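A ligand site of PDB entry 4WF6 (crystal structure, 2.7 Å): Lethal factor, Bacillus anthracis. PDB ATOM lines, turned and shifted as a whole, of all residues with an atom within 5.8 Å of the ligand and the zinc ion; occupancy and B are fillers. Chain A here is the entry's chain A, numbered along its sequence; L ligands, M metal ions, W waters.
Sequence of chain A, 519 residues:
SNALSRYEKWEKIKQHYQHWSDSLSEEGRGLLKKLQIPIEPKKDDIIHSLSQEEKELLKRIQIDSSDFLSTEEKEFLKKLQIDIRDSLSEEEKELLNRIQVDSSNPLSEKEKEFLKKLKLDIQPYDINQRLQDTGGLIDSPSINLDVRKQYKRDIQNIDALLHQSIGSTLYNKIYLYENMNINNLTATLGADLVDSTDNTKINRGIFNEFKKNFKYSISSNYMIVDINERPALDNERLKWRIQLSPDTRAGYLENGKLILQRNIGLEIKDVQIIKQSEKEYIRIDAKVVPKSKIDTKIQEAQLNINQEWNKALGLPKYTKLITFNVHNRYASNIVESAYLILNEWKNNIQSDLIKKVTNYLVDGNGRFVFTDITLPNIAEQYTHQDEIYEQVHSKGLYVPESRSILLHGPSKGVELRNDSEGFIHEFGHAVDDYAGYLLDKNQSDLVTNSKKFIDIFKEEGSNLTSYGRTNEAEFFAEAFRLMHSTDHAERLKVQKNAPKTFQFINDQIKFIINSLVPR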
ATOM      1  N   ASP A  67      11.979  -8.161  -2.052  1.00  0.00           N
ATOM      2  CA  ASP A  67      11.674  -9.558  -1.743  1.00  0.00           C
ATOM      3  C   ASP A  67      11.088  -9.716  -0.342  1.00  0.00           C
ATOM      4  O   ASP A  67      11.172 -10.796   0.251  1.00  0.00           O
ATOM      5  CB  ASP A  67      12.937 -10.409  -1.886  1.00  0.00           C
ATOM      6  CG  ASP A  67      14.064  -9.944  -0.972  1.00  0.00           C
ATOM      7  OD1 ASP A  67      14.057  -8.748  -0.587  1.00  0.00           O
ATOM      8  OD2 ASP A  67      14.948 -10.752  -0.651  1.00  0.00           O
ATOM      9  N   PHE A  68      10.487  -8.657   0.173  1.00  0.00           N
ATOM     10  CA  PHE A  68       9.976  -8.653   1.540  1.00  0.00           C
ATOM     11  C   PHE A  68       8.601  -8.010   1.642  1.00  0.00           C
ATOM     12  O   PHE A  68       7.922  -8.120   2.665  1.00  0.00           O
ATOM     13  CB  PHE A  68      10.951  -7.928   2.474  1.00  0.00           C
ATOM     14  CG  PHE A  68      11.285  -6.539   2.032  1.00  0.00           C
ATOM     15  CD1 PHE A  68      10.613  -5.449   2.568  1.00  0.00           C
ATOM     16  CD2 PHE A  68      12.286  -6.312   1.095  1.00  0.00           C
ATOM     17  CE1 PHE A  68      10.925  -4.158   2.169  1.00  0.00           C
ATOM     18  CE2 PHE A  68      12.598  -5.020   0.696  1.00  0.00           C
ATOM     19  CZ  PHE A  68      11.924  -3.953   1.231  1.00  0.00           C
ATOM     20  N   VAL A 392       9.443  -9.843   7.458  1.00  0.00           N
ATOM     21  CA  VAL A 392       9.472 -10.214   6.046  1.00  0.00           C
ATOM     22  C   VAL A 392       8.296 -11.080   5.657  1.00  0.00           C
ATOM     23  O   VAL A 392       7.991 -12.070   6.336  1.00  0.00           O
ATOM     24  CB  VAL A 392      10.771 -10.968   5.701  1.00  0.00           C
ATOM     25  CG1 VAL A 392      10.740 -11.447   4.260  1.00  0.00           C
ATOM     26  CG2 VAL A 392      11.989 -10.092   5.967  1.00  0.00           C
ATOM     27  N   SER A 394       7.235 -13.408   2.367  1.00  0.00           N
ATOM     28  CA  SER A 394       7.854 -13.993   1.195  1.00  0.00           C
ATOM     29  C   SER A 394       7.354 -15.413   1.006  1.00  0.00           C
ATOM     30  O   SER A 394       6.564 -15.910   1.814  1.00  0.00           O
ATOM     31  CB  SER A 394       9.379 -13.971   1.331  1.00  0.00           C
ATOM     32  OG  SER A 394       9.788 -14.568   2.553  1.00  0.00           O
ATOM     33  N   LYS A 395       7.798 -16.062  -0.061  1.00  0.00           N
ATOM     34  CA  LYS A 395       7.451 -17.459  -0.310  1.00  0.00           C
ATOM     35  C   LYS A 395       7.884 -18.329   0.853  1.00  0.00           C
ATOM     36  O   LYS A 395       7.101 -19.124   1.387  1.00  0.00           O
ATOM     37  CB  LYS A 395       8.088 -17.953  -1.607  1.00  0.00           C
ATOM     38  CG  LYS A 395       7.841 -19.422  -1.896  1.00  0.00           C
ATOM     39  CD  LYS A 395       6.357 -19.707  -2.014  1.00  0.00           C
ATOM     40  CE  LYS A 395       6.089 -21.181  -2.245  1.00  0.00           C
ATOM     41  NZ  LYS A 395       4.640 -21.448  -2.444  1.00  0.00           N
ATOM     42  N   GLY A 396       9.140 -18.163   1.253  1.00  0.00           N
ATOM     43  CA  GLY A 396       9.712 -18.959   2.330  1.00  0.00           C
ATOM     44  C   GLY A 396      10.689 -18.155   3.152  1.00  0.00           C
ATOM     45  O   GLY A 396      11.085 -17.048   2.755  1.00  0.00           O
ATOM     46  N   LEU A 397      11.080 -18.704   4.298  1.00  0.00           N
ATOM     47  CA  LEU A 397      11.949 -17.990   5.218  1.00  0.00           C
ATOM     48  C   LEU A 397      12.612 -18.950   6.202  1.00  0.00           C
ATOM     49  O   LEU A 397      12.014 -19.941   6.617  1.00  0.00           O
ATOM     50  CB  LEU A 397      11.159 -16.925   5.981  1.00  0.00           C
ATOM     51  CG  LEU A 397      11.929 -15.762   6.594  1.00  0.00           C
ATOM     52  CD1 LEU A 397      12.632 -14.970   5.501  1.00  0.00           C
ATOM     53  CD2 LEU A 397      10.988 -14.864   7.379  1.00  0.00           C
ATOM     54  N   TYR A 398      13.868 -18.675   6.545  1.00  0.00           N
ATOM     55  CA  TYR A 398      14.504 -19.377   7.651  1.00  0.00           C
ATOM     56  C   TYR A 398      14.816 -18.387   8.771  1.00  0.00           C
ATOM     57  O   TYR A 398      15.429 -17.339   8.541  1.00  0.00           O
ATOM     58  CB  TYR A 398      15.782 -20.082   7.220  1.00  0.00           C
ATOM     59  CG  TYR A 398      16.526 -20.711   8.384  1.00  0.00           C
ATOM     60  CD1 TYR A 398      16.006 -21.826   9.031  1.00  0.00           C
ATOM     61  CD2 TYR A 398      17.717 -20.180   8.848  1.00  0.00           C
ATOM     62  CE1 TYR A 398      16.668 -22.407  10.104  1.00  0.00           C
ATOM     63  CE2 TYR A 398      18.384 -20.753   9.920  1.00  0.00           C
ATOM     64  CZ  TYR A 398      17.848 -21.861  10.541  1.00  0.00           C
ATOM     65  OH  TYR A 398      18.510 -22.443  11.614  1.00  0.00           O
ATOM     66  N   LYS A 412       4.304 -17.446  -4.747  1.00  0.00           N
ATOM     67  CA  LYS A 412       5.299 -18.041  -5.637  1.00  0.00           C
ATOM     68  C   LYS A 412       6.635 -17.316  -5.523  1.00  0.00           C
ATOM     69  O   LYS A 412       6.693 -16.093  -5.630  1.00  0.00           O
ATOM     70  CB  LYS A 412       4.811 -18.011  -7.090  1.00  0.00           C
ATOM     71  CG  LYS A 412       5.704 -18.753  -8.073  1.00  0.00           C
ATOM     72  N   GLY A 413       7.697 -18.071  -5.277  1.00  0.00           N
ATOM     73  CA  GLY A 413       9.027 -17.494  -5.169  1.00  0.00           C
ATOM     74  C   GLY A 413       9.586 -17.155  -6.533  1.00  0.00           C
ATOM     75  O   GLY A 413       9.048 -17.582  -7.559  1.00  0.00           O
ATOM     76  N   VAL A 414      10.656 -16.365  -6.564  1.00  0.00           N
ATOM     77  CA  VAL A 414      11.263 -15.975  -7.825  1.00  0.00           C
ATOM     78  C   VAL A 414      11.923 -17.177  -8.508  1.00  0.00           C
ATOM     79  O   VAL A 414      12.658 -17.939  -7.886  1.00  0.00           O
ATOM     80  CB  VAL A 414      12.301 -14.834  -7.646  1.00  0.00           C
ATOM     81  CG1 VAL A 414      11.621 -13.569  -7.121  1.00  0.00           C
ATOM     82  CG2 VAL A 414      13.427 -15.253  -6.709  1.00  0.00           C
ATOM     83  N   LEU A 416      11.124 -20.130  -9.326  1.00  0.00           N
ATOM     84  CA  LEU A 416      10.975 -21.476  -8.787  1.00  0.00           C
ATOM     85  C   LEU A 416       9.918 -22.244  -9.587  1.00  0.00           C
ATOM     86  O   LEU A 416       8.985 -21.660 -10.112  1.00  0.00           O
ATOM     87  CB  LEU A 416      10.585 -21.424  -7.305  1.00  0.00           C
ATOM     88  CG  LEU A 416      11.584 -20.746  -6.359  1.00  0.00           C
ATOM     89  CD1 LEU A 416      11.119 -20.863  -4.916  1.00  0.00           C
ATOM     90  CD2 LEU A 416      12.977 -21.326  -6.524  1.00  0.00           C
ATOM     91  N   GLU A 421      11.207 -26.686  -4.293  1.00  0.00           N
ATOM     92  CA  GLU A 421      12.437 -25.957  -4.596  1.00  0.00           C
ATOM     93  C   GLU A 421      12.641 -24.827  -3.597  1.00  0.00           C
ATOM     94  O   GLU A 421      13.770 -24.481  -3.258  1.00  0.00           O
ATOM     95  CB  GLU A 421      12.414 -25.402  -6.015  1.00  0.00           C
ATOM     96  CG  GLU A 421      12.635 -26.444  -7.092  1.00  0.00           C
ATOM     97  CD  GLU A 421      12.945 -25.827  -8.441  1.00  0.00           C
ATOM     98  OE1 GLU A 421      12.670 -24.621  -8.626  1.00  0.00           O
ATOM     99  OE2 GLU A 421      13.468 -26.557  -9.315  1.00  0.00           O
ATOM    100  N   GLY A 422      11.536 -24.260  -3.114  1.00  0.00           N
ATOM    101  CA  GLY A 422      11.608 -23.207  -2.124  1.00  0.00           C
ATOM    102  C   GLY A 422      12.062 -23.711  -0.766  1.00  0.00           C
ATOM    103  O   GLY A 422      12.881 -23.077  -0.105  1.00  0.00           O
ATOM    104  N   HIS A 425      15.773 -24.419  -0.607  1.00  0.00           N
ATOM    105  CA  HIS A 425      16.458 -23.149  -0.422  1.00  0.00           C
ATOM    106  C   HIS A 425      16.549 -22.791   1.061  1.00  0.00           C
ATOM    107  O   HIS A 425      17.605 -22.378   1.545  1.00  0.00           O
ATOM    108  CB  HIS A 425      15.730 -22.038  -1.195  1.00  0.00           C
ATOM    109  CG  HIS A 425      16.223 -20.660  -0.903  1.00  0.00           C
ATOM    110  ND1 HIS A 425      16.971 -19.930  -1.793  1.00  0.00           N
ATOM    111  CD2 HIS A 425      16.040 -19.858   0.174  1.00  0.00           C
ATOM    112  CE1 HIS A 425      17.249 -18.742  -1.276  1.00  0.00           C
ATOM    113  NE2 HIS A 425      16.699 -18.677  -0.083  1.00  0.00           N
ATOM    114  N   GLU A 426      15.430 -22.942   1.764  1.00  0.00           N
ATOM    115  CA  GLU A 426      15.382 -22.583   3.179  1.00  0.00           C
ATOM    116  C   GLU A 426      16.214 -23.550   4.015  1.00  0.00           C
ATOM    117  O   GLU A 426      16.850 -23.137   4.993  1.00  0.00           O
ATOM    118  CB  GLU A 426      13.936 -22.559   3.676  1.00  0.00           C
ATOM    119  CG  GLU A 426      12.975 -21.767   2.795  1.00  0.00           C
ATOM    120  CD  GLU A 426      13.380 -20.308   2.617  1.00  0.00           C
ATOM    121  OE1 GLU A 426      12.879 -19.678   1.669  1.00  0.00           O
ATOM    122  OE2 GLU A 426      14.187 -19.803   3.420  1.00  0.00           O
ATOM    123  N   HIS A 429      19.676 -22.462   4.152  1.00  0.00           N
ATOM    124  CA  HIS A 429      19.949 -21.481   5.199  1.00  0.00           C
ATOM    125  C   HIS A 429      20.252 -22.168   6.528  1.00  0.00           C
ATOM    126  O   HIS A 429      21.108 -21.704   7.296  1.00  0.00           O
ATOM    127  CB  HIS A 429      18.763 -20.532   5.368  1.00  0.00           C
ATOM    128  CG  HIS A 429      18.616 -19.529   4.260  1.00  0.00           C
ATOM    129  ND1 HIS A 429      19.653 -18.727   3.845  1.00  0.00           N
ATOM    130  CD2 HIS A 429      17.546 -19.204   3.501  1.00  0.00           C
ATOM    131  CE1 HIS A 429      19.230 -17.947   2.862  1.00  0.00           C
ATOM    132  NE2 HIS A 429      17.956 -18.211   2.639  1.00  0.00           N
ATOM    133  N   TYR A 467      18.676 -13.833  -8.230  1.00  0.00           N
ATOM    134  CA  TYR A 467      18.351 -13.676  -6.822  1.00  0.00           C
ATOM    135  C   TYR A 467      19.551 -14.026  -5.933  1.00  0.00           C
ATOM    136  O   TYR A 467      19.679 -13.522  -4.827  1.00  0.00           O
ATOM    137  CB  TYR A 467      17.143 -14.535  -6.427  1.00  0.00           C
ATOM    138  CG  TYR A 467      16.749 -14.347  -4.990  1.00  0.00           C
ATOM    139  CD1 TYR A 467      16.129 -13.172  -4.568  1.00  0.00           C
ATOM    140  CD2 TYR A 467      17.014 -15.317  -4.036  1.00  0.00           C
ATOM    141  CE1 TYR A 467      15.774 -12.984  -3.244  1.00  0.00           C
ATOM    142  CE2 TYR A 467      16.665 -15.143  -2.704  1.00  0.00           C
ATOM    143  CZ  TYR A 467      16.046 -13.972  -2.314  1.00  0.00           C
ATOM    144  OH  TYR A 467      15.693 -13.775  -1.001  1.00  0.00           O
ATOM    145  N   GLU A 474      21.977 -15.580   0.605  1.00  0.00           N
ATOM    146  CA  GLU A 474      21.050 -16.041  -0.413  1.00  0.00           C
ATOM    147  C   GLU A 474      21.773 -16.782  -1.526  1.00  0.00           C
ATOM    148  O   GLU A 474      21.230 -17.714  -2.117  1.00  0.00           O
ATOM    149  CB  GLU A 474      20.239 -14.863  -0.986  1.00  0.00           C
ATOM    150  CG  GLU A 474      19.504 -14.029   0.063  1.00  0.00           C
ATOM    151  CD  GLU A 474      18.387 -14.790   0.780  1.00  0.00           C
ATOM    152  OE1 GLU A 474      17.821 -14.234   1.740  1.00  0.00           O
ATOM    153  OE2 GLU A 474      18.073 -15.934   0.378  1.00  0.00           O
ATOM    154  N   ALA A 477      22.371 -20.197  -0.467  1.00  0.00           N
ATOM    155  CA  ALA A 477      21.091 -20.892  -0.449  1.00  0.00           C
ATOM    156  C   ALA A 477      20.644 -21.261  -1.859  1.00  0.00           C
ATOM    157  O   ALA A 477      20.112 -22.356  -2.077  1.00  0.00           O
ATOM    158  CB  ALA A 477      20.044 -20.038   0.227  1.00  0.00           C
ATOM    159  N   GLU A 478      20.862 -20.366  -2.809  1.00  0.00           N
ATOM    160  CA  GLU A 478      20.515 -20.616  -4.198  1.00  0.00           C
ATOM    161  C   GLU A 478      21.415 -21.691  -4.804  1.00  0.00           C
ATOM    162  O   GLU A 478      20.955 -22.589  -5.508  1.00  0.00           O
ATOM    163  CB  GLU A 478      20.607 -19.326  -5.025  1.00  0.00           C
ATOM    164  CG  GLU A 478      19.393 -18.411  -4.882  1.00  0.00           C
ATOM    165  CD  GLU A 478      18.125 -19.015  -5.464  1.00  0.00           C
ATOM    166  OE1 GLU A 478      17.758 -18.652  -6.604  1.00  0.00           O
ATOM    167  OE2 GLU A 478      17.498 -19.859  -4.787  1.00  0.00           O
ATOM    168  N   ARG A 481      20.378 -24.859  -3.447  1.00  0.00           N
ATOM    169  CA  ARG A 481      19.139 -25.257  -4.099  1.00  0.00           C
ATOM    170  C   ARG A 481      19.436 -25.975  -5.410  1.00  0.00           C
ATOM    171  O   ARG A 481      19.005 -27.103  -5.625  1.00  0.00           O
ATOM    172  CB  ARG A 481      18.262 -24.030  -4.342  1.00  0.00           C
ATOM    173  CG  ARG A 481      16.930 -24.354  -5.009  1.00  0.00           C
ATOM    174  CD  ARG A 481      16.027 -23.130  -5.089  1.00  0.00           C
ATOM    175  NE  ARG A 481      16.543 -22.085  -5.977  1.00  0.00           N
ATOM    176  CZ  ARG A 481      16.363 -22.087  -7.296  1.00  0.00           C
ATOM    177  NH1 ARG A 481      15.705 -23.069  -7.890  1.00  0.00           N
ATOM    178  NH2 ARG A 481      16.856 -21.094  -8.035  1.00  0.00           N
HETATM  179  C1  LIG L   1      13.974 -15.825   1.217  1.00  0.00           C
HETATM  180  C2  LIG L   1      12.977 -14.795   0.759  1.00  0.00           C
HETATM  181  N1  LIG L   1      13.700 -16.501   2.316  1.00  0.00           N
HETATM  182  O1  LIG L   1      14.998 -16.006   0.576  1.00  0.00           O
HETATM  183  O2  LIG L   1      14.595 -17.475   2.761  1.00  0.00           O
HETATM  184  C3  LIG L   1      13.311 -13.444   1.382  1.00  0.00           C
HETATM  185  N2  LIG L   1      12.944 -14.709  -0.688  1.00  0.00           N
HETATM  186  S1  LIG L   1      11.875 -15.566  -1.510  1.00  0.00           S
HETATM  187  O3  LIG L   1      11.408 -14.811  -2.637  1.00  0.00           O
HETATM  188  O4  LIG L   1      10.755 -15.908  -0.670  1.00  0.00           O
HETATM  189  C4  LIG L   1      12.570 -16.909  -2.031  1.00  0.00           C
HETATM  190  C5  LIG L   1      13.340 -16.898  -3.197  1.00  0.00           C
HETATM  191  C6  LIG L   1      13.923 -18.089  -3.631  1.00  0.00           C
HETATM  192  C7  LIG L   1      13.744 -19.262  -2.930  1.00  0.00           C
HETATM  193  C8  LIG L   1      12.971 -19.272  -1.774  1.00  0.00           C
HETATM  194  C9  LIG L   1      12.378 -18.099  -1.339  1.00  0.00           C
HETATM  195  F1  LIG L   1      14.310 -20.397  -3.368  1.00  0.00           F
HETATM  196  C10 LIG L   1      14.765 -18.094  -4.888  1.00  0.00           C
HETATM  197 ZN    ZN M   1      16.616 -16.974   1.442  1.00  0.00          ZN
HETATM  198  O   HOH W   1      15.721 -17.938  -8.064  1.00  0.00           O
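The side-chain carboxylate (OE1) of Glu 426 sits at hydrogen-bond distance from a nitrogen (N1) of the ligand (3.3 Å).
A nitrogen (N1) of the ligand lies within hydrogen-bond range of the backbone carbonyl oxygen of Gly 396 (2.7 Å).
O4 of the ligand sits at hydrogen-bond distance from N of Gly 396 (3.4 Å).
O4 of the ligand lies within hydrogen-bond range of N of Lys 395 (3.0 Å).
The side-chain hydroxyl (OH) of Tyr 467 sits at hydrogen-bond distance from a nitrogen (N2) of the ligand, 2.9 Å away.
The side-chain carboxylate (OE2) of Glu 426 sits at hydrogen-bond distance from the backbone NH (N) of Tyr 398.
The backbone carbonyl oxygen (O) of Gly 396 is in hydrogen-bond range of the side-chain hydroxyl (OG) of Ser 394, at 2.8 Å.
A ring nitrogen (ND1) of His 425 is in hydrogen-bond range of the side-chain carboxylate (OE2) of Glu 478, at 3.0 Å.
The guanidinium group (NH1) of Arg 481 lies within salt-bridge range of the side-chain carboxylate (OE1) of Glu 421.
The side-chain carboxylate of Glu 478 lies within salt-bridge range of the guanidinium group of Arg 481, 2.7 Å away.
N of Leu 397 sits close to OE1 of Glu 426 (3.3 Å).
The side-chain carboxylate (OD2) of Asp 67 sits at hydrogen-bond distance from the side-chain hydroxyl (OH) of Tyr 467 (3.1 Å).
OH of Tyr 467 sits close to OE2 of Glu 474 (3.5 Å).
Merely in contact with the ligand: Ser 394 (3.1 Å), Glu 478 (3.3 Å), Leu 416 (3.5 Å), Asp 67 (3.6 Å), Val 414 (3.6 Å), Leu 397 (3.6 Å) and Arg 481 (3.7 Å).
Hydrophobic or aromatic side chains that line the ligand: Leu 397, Val 414, Leu 416, His 425, His 429 and Tyr 467.
The nearest printed residue that does not touch the ligand is Tyr 398 (4.04 Å).
Of the 22 residues printed, 3 come within 4 Å of the zinc ion.
Along chain A the residues within 4 Å of the zinc ion span positions 425 to 474.
O1 of the ligand binds the zinc ion, 2.1 Å away.
The side-chain carboxylate (OE2) of Glu 474 binds the zinc ion (2.1 Å).
The zinc ion is bound by NE2 of His 429.
A ring nitrogen (NE2) of His 425 binds the zinc ion (2.3 Å).
O2 of the ligand binds the zinc ion.
The zinc ion has five donor atoms within binding distance.
Water W1 lies within hydrogen-bond range of OE1 of Glu 478 (2.6 Å), O of Val 414 (3.1 Å) and NH2 of Arg 481 (3.4 Å).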
